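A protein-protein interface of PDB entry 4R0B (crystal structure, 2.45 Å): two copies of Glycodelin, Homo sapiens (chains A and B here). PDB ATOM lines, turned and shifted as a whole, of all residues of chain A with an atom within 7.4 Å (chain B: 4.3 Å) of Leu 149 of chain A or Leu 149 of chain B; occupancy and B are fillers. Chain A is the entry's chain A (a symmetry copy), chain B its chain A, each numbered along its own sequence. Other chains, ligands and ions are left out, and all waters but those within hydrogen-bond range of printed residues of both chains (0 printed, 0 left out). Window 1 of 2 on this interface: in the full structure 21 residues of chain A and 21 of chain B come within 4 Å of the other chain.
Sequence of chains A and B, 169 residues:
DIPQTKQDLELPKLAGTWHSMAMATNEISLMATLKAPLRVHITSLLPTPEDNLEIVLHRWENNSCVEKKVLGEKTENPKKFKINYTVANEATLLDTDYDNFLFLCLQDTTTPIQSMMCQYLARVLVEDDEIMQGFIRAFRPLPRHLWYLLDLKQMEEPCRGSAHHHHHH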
ATOM      1  N   ALA A  22      10.841   2.487 -14.820  1.00  0.00           N
ATOM      2  CA  ALA A  22      11.366   3.076 -13.598  1.00  0.00           C
ATOM      3  C   ALA A  22      11.682   4.542 -13.814  1.00  0.00           C
ATOM      4  O   ALA A  22      11.784   4.990 -14.947  1.00  0.00           O
ATOM      5  CB  ALA A  22      12.621   2.336 -13.154  1.00  0.00           C
ATOM      6  N   MET A  23      11.839   5.283 -12.725  1.00  0.00           N
ATOM      7  CA  MET A  23      12.192   6.700 -12.791  1.00  0.00           C
ATOM      8  C   MET A  23      13.200   7.017 -11.705  1.00  0.00           C
ATOM      9  O   MET A  23      13.109   6.496 -10.595  1.00  0.00           O
ATOM     10  CB  MET A  23      10.978   7.599 -12.544  1.00  0.00           C
ATOM     11  CG  MET A  23       9.705   7.193 -13.249  1.00  0.00           C
ATOM     12  SD  MET A  23       8.278   8.120 -12.648  1.00  0.00           S
ATOM     13  CE  MET A  23       8.828   9.821 -12.814  1.00  0.00           C
ATOM     14  N   ALA A  24      14.130   7.912 -12.011  1.00  0.00           N
ATOM     15  CA  ALA A  24      15.111   8.308 -11.026  1.00  0.00           C
ATOM     16  C   ALA A  24      15.251   9.812 -10.992  1.00  0.00           C
ATOM     17  O   ALA A  24      15.065  10.490 -12.007  1.00  0.00           O
ATOM     18  CB  ALA A  24      16.452   7.638 -11.306  1.00  0.00           C
ATOM     19  N   THR A  25      15.558  10.328  -9.807  1.00  0.00           N
ATOM     20  CA  THR A  25      15.820  11.742  -9.645  1.00  0.00           C
ATOM     21  C   THR A  25      16.880  12.001  -8.579  1.00  0.00           C
ATOM     22  O   THR A  25      17.089  11.188  -7.682  1.00  0.00           O
ATOM     23  CB  THR A  25      14.530  12.507  -9.295  1.00  0.00           C
ATOM     24  OG1 THR A  25      14.767  13.920  -9.398  1.00  0.00           O
ATOM     25  CG2 THR A  25      14.055  12.163  -7.885  1.00  0.00           C
ATOM     26  N   ILE A  28      14.185  14.465  -4.783  1.00  0.00           N
ATOM     27  CA  ILE A  28      13.012  13.629  -4.536  1.00  0.00           C
ATOM     28  C   ILE A  28      11.695  14.393  -4.765  1.00  0.00           C
ATOM     29  O   ILE A  28      10.742  13.824  -5.296  1.00  0.00           O
ATOM     30  CB  ILE A  28      13.092  12.938  -3.141  1.00  0.00           C
ATOM     31  CG1 ILE A  28      11.856  12.070  -2.870  1.00  0.00           C
ATOM     32  CG2 ILE A  28      13.333  13.938  -2.016  1.00  0.00           C
ATOM     33  CD1 ILE A  28      11.664  10.951  -3.874  1.00  0.00           C
ATOM     34  N   MET A  31       9.481  14.426  -7.938  1.00  0.00           N
ATOM     35  CA  MET A  31       8.940  13.145  -8.334  1.00  0.00           C
ATOM     36  C   MET A  31       8.068  12.473  -7.277  1.00  0.00           C
ATOM     37  O   MET A  31       7.306  11.571  -7.620  1.00  0.00           O
ATOM     38  CB  MET A  31      10.125  12.246  -8.641  1.00  0.00           C
ATOM     39  CG  MET A  31       9.801  11.008  -9.429  1.00  0.00           C
ATOM     40  SD  MET A  31      11.329  10.156  -9.850  1.00  0.00           S
ATOM     41  CE  MET A  31      11.757   9.336  -8.313  1.00  0.00           C
ATOM     42  N   CYS A 118      15.226  11.131 -14.777  1.00  0.00           N
ATOM     43  CA  CYS A 118      15.467  10.226 -15.899  1.00  0.00           C
ATOM     44  C   CYS A 118      14.523   9.050 -15.821  1.00  0.00           C
ATOM     45  O   CYS A 118      14.201   8.566 -14.743  1.00  0.00           O
ATOM     46  CB  CYS A 118      16.921   9.739 -15.953  1.00  0.00           C
ATOM     47  SG  CYS A 118      18.146  11.083 -16.079  1.00  0.00           S
ATOM     48  N   TYR A 120      13.474   5.199 -17.346  1.00  0.00           N
ATOM     49  CA  TYR A 120      13.783   3.952 -18.025  1.00  0.00           C
ATOM     50  C   TYR A 120      12.528   3.585 -18.796  1.00  0.00           C
ATOM     51  O   TYR A 120      11.522   3.142 -18.222  1.00  0.00           O
ATOM     52  CB  TYR A 120      14.198   2.900 -16.980  1.00  0.00           C
ATOM     53  CG  TYR A 120      14.187   1.444 -17.376  1.00  0.00           C
ATOM     54  CD1 TYR A 120      14.121   1.030 -18.719  1.00  0.00           C
ATOM     55  CD2 TYR A 120      14.272   0.464 -16.390  1.00  0.00           C
ATOM     56  CE1 TYR A 120      14.109  -0.321 -19.054  1.00  0.00           C
ATOM     57  CE2 TYR A 120      14.263  -0.880 -16.708  1.00  0.00           C
ATOM     58  CZ  TYR A 120      14.180  -1.272 -18.037  1.00  0.00           C
ATOM     59  OH  TYR A 120      14.181  -2.619 -18.337  1.00  0.00           O
ATOM     60  N   MET A 132      17.890  -2.819 -16.130  1.00  0.00           N
ATOM     61  CA  MET A 132      17.596  -2.097 -14.906  1.00  0.00           C
ATOM     62  C   MET A 132      18.907  -1.721 -14.232  1.00  0.00           C
ATOM     63  O   MET A 132      19.061  -0.622 -13.705  1.00  0.00           O
ATOM     64  CB  MET A 132      16.758  -2.950 -13.950  1.00  0.00           C
ATOM     65  CG  MET A 132      16.482  -2.286 -12.601  1.00  0.00           C
ATOM     66  SD  MET A 132      15.511  -0.764 -12.718  1.00  0.00           S
ATOM     67  CE  MET A 132      13.908  -1.491 -13.068  1.00  0.00           C
ATOM     68  N   PHE A 135      20.556   1.102 -16.121  1.00  0.00           N
ATOM     69  CA  PHE A 135      19.871   2.342 -15.756  1.00  0.00           C
ATOM     70  C   PHE A 135      20.469   2.959 -14.494  1.00  0.00           C
ATOM     71  O   PHE A 135      20.733   4.147 -14.457  1.00  0.00           O
ATOM     72  CB  PHE A 135      18.386   2.071 -15.530  1.00  0.00           C
ATOM     73  CG  PHE A 135      17.556   3.315 -15.275  1.00  0.00           C
ATOM     74  CD1 PHE A 135      17.602   4.404 -16.146  1.00  0.00           C
ATOM     75  CD2 PHE A 135      16.688   3.376 -14.188  1.00  0.00           C
ATOM     76  CE1 PHE A 135      16.815   5.528 -15.927  1.00  0.00           C
ATOM     77  CE2 PHE A 135      15.901   4.498 -13.969  1.00  0.00           C
ATOM     78  CZ  PHE A 135      15.965   5.575 -14.838  1.00  0.00           C
ATOM     79  N   ILE A 136      20.679   2.140 -13.474  1.00  0.00           N
ATOM     80  CA  ILE A 136      21.282   2.590 -12.234  1.00  0.00           C
ATOM     81  C   ILE A 136      22.725   3.020 -12.470  1.00  0.00           C
ATOM     82  O   ILE A 136      23.157   4.058 -11.989  1.00  0.00           O
ATOM     83  CB  ILE A 136      21.234   1.482 -11.167  1.00  0.00           C
ATOM     84  CG1 ILE A 136      19.779   1.234 -10.742  1.00  0.00           C
ATOM     85  CG2 ILE A 136      22.091   1.845  -9.961  1.00  0.00           C
ATOM     86  CD1 ILE A 136      19.582  -0.083 -10.014  1.00  0.00           C
ATOM     87  N   PHE A 139      22.975   6.738 -14.209  1.00  0.00           N
ATOM     88  CA  PHE A 139      22.883   7.914 -13.352  1.00  0.00           C
ATOM     89  C   PHE A 139      23.891   7.899 -12.185  1.00  0.00           C
ATOM     90  O   PHE A 139      23.968   8.848 -11.412  1.00  0.00           O
ATOM     91  CB  PHE A 139      21.418   8.183 -12.923  1.00  0.00           C
ATOM     92  CG  PHE A 139      20.788   7.128 -12.024  1.00  0.00           C
ATOM     93  CD1 PHE A 139      21.255   6.894 -10.719  1.00  0.00           C
ATOM     94  CD2 PHE A 139      19.653   6.433 -12.440  1.00  0.00           C
ATOM     95  CE1 PHE A 139      20.644   5.954  -9.888  1.00  0.00           C
ATOM     96  CE2 PHE A 139      19.038   5.494 -11.601  1.00  0.00           C
ATOM     97  CZ  PHE A 139      19.533   5.260 -10.329  1.00  0.00           C
ATOM     98  N   TRP A 147      20.742   9.367  -5.179  1.00  0.00           N
ATOM     99  CA  TRP A 147      19.714   9.283  -6.199  1.00  0.00           C
ATOM    100  C   TRP A 147      18.541   8.479  -5.700  1.00  0.00           C
ATOM    101  O   TRP A 147      18.712   7.461  -5.034  1.00  0.00           O
ATOM    102  CB  TRP A 147      20.267   8.652  -7.473  1.00  0.00           C
ATOM    103  CG  TRP A 147      20.809   9.668  -8.397  1.00  0.00           C
ATOM    104  CD1 TRP A 147      21.984  10.349  -8.266  1.00  0.00           C
ATOM    105  CD2 TRP A 147      20.191  10.154  -9.591  1.00  0.00           C
ATOM    106  NE1 TRP A 147      22.143  11.224  -9.312  1.00  0.00           N
ATOM    107  CE2 TRP A 147      21.057  11.124 -10.143  1.00  0.00           C
ATOM    108  CE3 TRP A 147      18.997   9.860 -10.258  1.00  0.00           C
ATOM    109  CZ2 TRP A 147      20.765  11.804 -11.337  1.00  0.00           C
ATOM    110  CZ3 TRP A 147      18.706  10.538 -11.448  1.00  0.00           C
ATOM    111  CH2 TRP A 147      19.588  11.497 -11.972  1.00  0.00           C
ATOM    112  N   TYR A 148      17.348   8.955  -6.023  1.00  0.00           N
ATOM    113  CA  TYR A 148      16.145   8.243  -5.683  1.00  0.00           C
ATOM    114  C   TYR A 148      15.648   7.541  -6.921  1.00  0.00           C
ATOM    115  O   TYR A 148      15.792   8.033  -8.038  1.00  0.00           O
ATOM    116  CB  TYR A 148      15.081   9.189  -5.149  1.00  0.00           C
ATOM    117  CG  TYR A 148      15.407   9.763  -3.808  1.00  0.00           C
ATOM    118  CD1 TYR A 148      16.161  10.922  -3.703  1.00  0.00           C
ATOM    119  CD2 TYR A 148      14.954   9.158  -2.636  1.00  0.00           C
ATOM    120  CE1 TYR A 148      16.453  11.469  -2.472  1.00  0.00           C
ATOM    121  CE2 TYR A 148      15.242   9.697  -1.395  1.00  0.00           C
ATOM    122  CZ  TYR A 148      15.998  10.850  -1.323  1.00  0.00           C
ATOM    123  OH  TYR A 148      16.307  11.412  -0.100  1.00  0.00           O
ATOM    124  N   LEU A 149      15.067   6.375  -6.709  1.00  0.00           N
ATOM    125  CA  LEU A 149      14.592   5.557  -7.788  1.00  0.00           C
ATOM    126  C   LEU A 149      13.191   5.095  -7.427  1.00  0.00           C
ATOM    127  O   LEU A 149      12.963   4.597  -6.333  1.00  0.00           O
ATOM    128  CB  LEU A 149      15.519   4.362  -7.957  1.00  0.00           C
ATOM    129  CG  LEU A 149      15.281   3.523  -9.215  1.00  0.00           C
ATOM    130  CD1 LEU A 149      16.306   3.896 -10.277  1.00  0.00           C
ATOM    131  CD2 LEU A 149      15.341   2.031  -8.895  1.00  0.00           C
ATOM    132  N   LEU A 150      12.254   5.275  -8.347  1.00  0.00           N
ATOM    133  CA  LEU A 150      10.901   4.786  -8.173  1.00  0.00           C
ATOM    134  C   LEU A 150      10.716   3.606  -9.106  1.00  0.00           C
ATOM    135  O   LEU A 150      10.847   3.755 -10.307  1.00  0.00           O
ATOM    136  CB  LEU A 150       9.921   5.909  -8.502  1.00  0.00           C
ATOM    137  CG  LEU A 150       8.425   5.606  -8.493  1.00  0.00           C
ATOM    138  CD1 LEU A 150       7.948   4.952  -7.201  1.00  0.00           C
ATOM    139  CD2 LEU A 150       7.697   6.914  -8.759  1.00  0.00           C
ATOM    140  N   ASP A 151      10.462   2.426  -8.547  1.00  0.00           N
ATOM    141  CA  ASP A 151      10.277   1.207  -9.337  1.00  0.00           C
ATOM    142  C   ASP A 151       8.775   0.954  -9.513  1.00  0.00           C
ATOM    143  O   ASP A 151       8.068   0.644  -8.551  1.00  0.00           O
ATOM    144  CB  ASP A 151      10.972   0.015  -8.668  1.00  0.00           C
ATOM    145  CG  ASP A 151      10.839  -1.292  -9.481  1.00  0.00           C
ATOM    146  OD1 ASP A 151      10.848  -1.246 -10.739  1.00  0.00           O
ATOM    147  OD2 ASP A 151      10.732  -2.379  -8.860  1.00  0.00           O
ATOM    148  N   LEU A 152       8.303   1.096 -10.752  1.00  0.00           N
ATOM    149  CA  LEU A 152       6.868   1.173 -11.054  1.00  0.00           C
ATOM    150  C   LEU A 152       6.234  -0.200 -11.121  1.00  0.00           C
ATOM    151  O   LEU A 152       6.933  -1.205 -11.216  1.00  0.00           O
ATOM    152  CB  LEU A 152       6.639   1.907 -12.381  1.00  0.00           C
ATOM    153  CG  LEU A 152       7.208   3.329 -12.474  1.00  0.00           C
ATOM    154  CD1 LEU A 152       7.205   3.825 -13.913  1.00  0.00           C
ATOM    155  CD2 LEU A 152       6.435   4.287 -11.579  1.00  0.00           C
ATOM    156  N   MET B  23      18.717   1.661   0.253  1.00  0.00           N
ATOM    157  CA  MET B  23      17.545   1.558   1.120  1.00  0.00           C
ATOM    158  C   MET B  23      16.288   1.639   0.277  1.00  0.00           C
ATOM    159  O   MET B  23      16.228   2.402  -0.686  1.00  0.00           O
ATOM    160  CB  MET B  23      17.479   2.712   2.124  1.00  0.00           C
ATOM    161  CG  MET B  23      18.781   3.071   2.800  1.00  0.00           C
ATOM    162  SD  MET B  23      18.662   4.624   3.710  1.00  0.00           S
ATOM    163  CE  MET B  23      17.222   4.350   4.747  1.00  0.00           C
ATOM    164  N   ALA B  24      15.267   0.891   0.672  1.00  0.00           N
ATOM    165  CA  ALA B  24      14.014   0.931  -0.048  1.00  0.00           C
ATOM    166  C   ALA B  24      12.855   1.061   0.914  1.00  0.00           C
ATOM    167  O   ALA B  24      12.917   0.582   2.051  1.00  0.00           O
ATOM    168  CB  ALA B  24      13.861  -0.304  -0.928  1.00  0.00           C
ATOM    169  N   PHE B 135      18.280  -7.436  -4.444  1.00  0.00           N
ATOM    170  CA  PHE B 135      17.625  -6.529  -3.500  1.00  0.00           C
ATOM    171  C   PHE B 135      16.309  -5.994  -4.061  1.00  0.00           C
ATOM    172  O   PHE B 135      15.304  -5.993  -3.374  1.00  0.00           O
ATOM    173  CB  PHE B 135      18.549  -5.357  -3.178  1.00  0.00           C
ATOM    174  CG  PHE B 135      18.020  -4.423  -2.105  1.00  0.00           C
ATOM    175  CD1 PHE B 135      17.600  -4.910  -0.868  1.00  0.00           C
ATOM    176  CD2 PHE B 135      17.992  -3.047  -2.316  1.00  0.00           C
ATOM    177  CE1 PHE B 135      17.148  -4.048   0.124  1.00  0.00           C
ATOM    178  CE2 PHE B 135      17.543  -2.184  -1.326  1.00  0.00           C
ATOM    179  CZ  PHE B 135      17.119  -2.685  -0.106  1.00  0.00           C
ATOM    180  N   PHE B 139      12.110  -7.057  -2.691  1.00  0.00           N
ATOM    181  CA  PHE B 139      10.958  -6.239  -2.333  1.00  0.00           C
ATOM    182  C   PHE B 139       9.902  -6.147  -3.451  1.00  0.00           C
ATOM    183  O   PHE B 139       8.854  -5.537  -3.274  1.00  0.00           O
ATOM    184  CB  PHE B 139      11.400  -4.867  -1.761  1.00  0.00           C
ATOM    185  CG  PHE B 139      12.111  -3.942  -2.740  1.00  0.00           C
ATOM    186  CD1 PHE B 139      11.452  -3.401  -3.856  1.00  0.00           C
ATOM    187  CD2 PHE B 139      13.417  -3.521  -2.490  1.00  0.00           C
ATOM    188  CE1 PHE B 139      12.101  -2.520  -4.723  1.00  0.00           C
ATOM    189  CE2 PHE B 139      14.063  -2.631  -3.359  1.00  0.00           C
ATOM    190  CZ  PHE B 139      13.403  -2.132  -4.470  1.00  0.00           C
ATOM    191  N   TRP B 147       7.595   1.136  -5.125  1.00  0.00           N
ATOM    192  CA  TRP B 147       8.670   1.146  -4.149  1.00  0.00           C
ATOM    193  C   TRP B 147       9.677   2.213  -4.487  1.00  0.00           C
ATOM    194  O   TRP B 147      10.016   2.415  -5.651  1.00  0.00           O
ATOM    195  CB  TRP B 147       9.358  -0.214  -4.089  1.00  0.00           C
ATOM    196  CG  TRP B 147       8.734  -1.100  -3.085  1.00  0.00           C
ATOM    197  CD1 TRP B 147       7.539  -1.748  -3.197  1.00  0.00           C
ATOM    198  CD2 TRP B 147       9.250  -1.423  -1.791  1.00  0.00           C
ATOM    199  NE1 TRP B 147       7.282  -2.467  -2.055  1.00  0.00           N
ATOM    200  CE2 TRP B 147       8.318  -2.286  -1.175  1.00  0.00           C
ATOM    201  CE3 TRP B 147      10.413  -1.079  -1.095  1.00  0.00           C
ATOM    202  CZ2 TRP B 147       8.515  -2.813   0.112  1.00  0.00           C
ATOM    203  CZ3 TRP B 147      10.609  -1.604   0.189  1.00  0.00           C
ATOM    204  CH2 TRP B 147       9.664  -2.461   0.775  1.00  0.00           C
ATOM    205  N   TYR B 148      10.146   2.900  -3.456  1.00  0.00           N
ATOM    206  CA  TYR B 148      11.175   3.890  -3.625  1.00  0.00           C
ATOM    207  C   TYR B 148      12.484   3.289  -3.183  1.00  0.00           C
ATOM    208  O   TYR B 148      12.539   2.481  -2.258  1.00  0.00           O
ATOM    209  CB  TYR B 148      10.869   5.143  -2.820  1.00  0.00           C
ATOM    210  CG  TYR B 148       9.700   5.919  -3.338  1.00  0.00           C
ATOM    211  CD1 TYR B 148       8.414   5.615  -2.922  1.00  0.00           C
ATOM    212  CD2 TYR B 148       9.876   6.968  -4.240  1.00  0.00           C
ATOM    213  CE1 TYR B 148       7.331   6.335  -3.381  1.00  0.00           C
ATOM    214  CE2 TYR B 148       8.797   7.697  -4.707  1.00  0.00           C
ATOM    215  CZ  TYR B 148       7.527   7.369  -4.277  1.00  0.00           C
ATOM    216  OH  TYR B 148       6.428   8.074  -4.728  1.00  0.00           O
ATOM    217  N   LEU B 149      13.544   3.688  -3.861  1.00  0.00           N
ATOM    218  CA  LEU B 149      14.854   3.167  -3.600  1.00  0.00           C
ATOM    219  C   LEU B 149      15.808   4.347  -3.523  1.00  0.00           C
ATOM    220  O   LEU B 149      15.815   5.198  -4.401  1.00  0.00           O
ATOM    221  CB  LEU B 149      15.257   2.231  -4.729  1.00  0.00           C
ATOM    222  CG  LEU B 149      16.526   1.414  -4.480  1.00  0.00           C
ATOM    223  CD1 LEU B 149      16.149   0.003  -4.052  1.00  0.00           C
ATOM    224  CD2 LEU B 149      17.412   1.390  -5.724  1.00  0.00           C
ATOM    225  N   LEU B 150      16.600   4.398  -2.462  1.00  0.00           N
ATOM    226  CA  LEU B 150      17.627   5.410  -2.317  1.00  0.00           C
ATOM    227  C   LEU B 150      18.969   4.735  -2.516  1.00  0.00           C
ATOM    228  O   LEU B 150      19.308   3.831  -1.774  1.00  0.00           O
ATOM    229  CB  LEU B 150      17.521   6.029  -0.926  1.00  0.00           C
ATOM    230  CG  LEU B 150      18.566   7.054  -0.495  1.00  0.00           C
ATOM    231  CD1 LEU B 150      18.738   8.199  -1.488  1.00  0.00           C
ATOM    232  CD2 LEU B 150      18.161   7.565   0.879  1.00  0.00           C
ATOM    233  N   ASP B 151      19.706   5.142  -3.545  1.00  0.00           N
ATOM    234  CA  ASP B 151      21.013   4.559  -3.853  1.00  0.00           C
ATOM    235  C   ASP B 151      22.107   5.467  -3.278  1.00  0.00           C
ATOM    236  O   ASP B 151      22.306   6.592  -3.743  1.00  0.00           O
ATOM    237  CB  ASP B 151      21.182   4.368  -5.366  1.00  0.00           C
ATOM    238  CG  ASP B 151      22.532   3.721  -5.743  1.00  0.00           C
ATOM    239  OD1 ASP B 151      23.038   2.850  -4.989  1.00  0.00           O
ATOM    240  OD2 ASP B 151      23.094   4.080  -6.808  1.00  0.00           O
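Among the printed residues, merely in contact across the chains: Tyr 148 of chain A with Leu 149 of chain B (3.3 Å), Leu 149 of chain A with Tyr 148 of chain B (3.3 Å), Leu 150 of chain A with Trp 147 of chain B (3.6 Å), Trp 147 of chain A with Leu 150 of chain B (3.6 Å), Leu 149 of chain A with Trp 147 of chain B (3.7 Å), Trp 147 of chain A with Leu 149 of chain B (3.7 Å), Tyr 148 of chain A with Leu 150 of chain B (3.8 Å), Leu 150 of chain A with Tyr 148 of chain B (3.8 Å) and Ile 136 of chain A with Asp 151 of chain B (3.99 Å).
Trp 147 of chain A touches Leu 150 of chain B, and with the chains exchanged Leu 150 of chain A touches Trp 147 of chain B.
Trp 147 of chain A touches Asp 151 of chain B, and with the chains exchanged Asp 151 of chain A touches Trp 147 of chain B.
Tyr 148 of chain A touches Leu 149 of chain B, and with the chains exchanged Leu 149 of chain A touches Tyr 148 of chain B.
Tyr 148 of chain A touches Leu 150 of chain B, and with the chains exchanged Leu 150 of chain A touches Tyr 148 of chain B.
Positions printed for both chains: 23, 24, 135, 139, 147, 148, 149, 150 and 151.
Of the 12 pairs that touch across the chains among the printed residues, 11 have their exchanged pair printed and touching as well.
The backbone carbonyl oxygen (O) of Trp 147 of chain B lies within hydrogen-bond range of the backbone NH (N) of Asp 151 of chain A, 2.9 Å away.
N of Leu 149 of chain B sits at hydrogen-bond distance from O of Leu 149 of chain A (2.7 Å).
The backbone NH (N) of Asp 151 of chain B is in hydrogen-bond range of the backbone carbonyl oxygen (O) of Trp 147 of chain A (2.9 Å).
Of the 18 printed residues of chain A, 6 touch a printed residue of chain B.
Printed residues of chain A that touch a printed residue of chain B: Ile 136, Trp 147, Tyr 148, Leu 149, Leu 150 and Asp 151.
Printed residues of chain B that touch a printed residue of chain A: Trp 147, Tyr 148, Leu 149, Leu 150 and Asp 151.
O of Met 23 of chain B is in hydrogen-bond range of N of Leu 150 of chain B, at 2.7 Å.
N of Leu 150 of chain A lies within hydrogen-bond range of O of Met 23 of chain A (2.7 Å).
N of Tyr 148 of chain A sits at hydrogen-bond distance from O of Thr 25 of chain A (2.8 Å).
Of chain B, only Trp 147, Tyr 148 and Leu 149 come within 4 Å of Leu 149 of chain A.
Printed residues of chain B within 4 Å of Leu 150 of chain A: Trp 147 (3.6 Å) and Tyr 148 (3.8 Å).
Of chain A, only Trp 147, Tyr 148 and Leu 149 come within 4 Å of Leu 149 of chain B.
Of the printed residues of chain A, Asp 151 of chain B touches Ile 136 and Trp 147.
The nearest printed residue of chain B that does not touch Leu 149 of chain A is Leu 150 of chain B (4.9 Å).
The nearest residue of chain A that does not touch Leu 149 of chain B is Leu 150 of chain A (4.9 Å).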
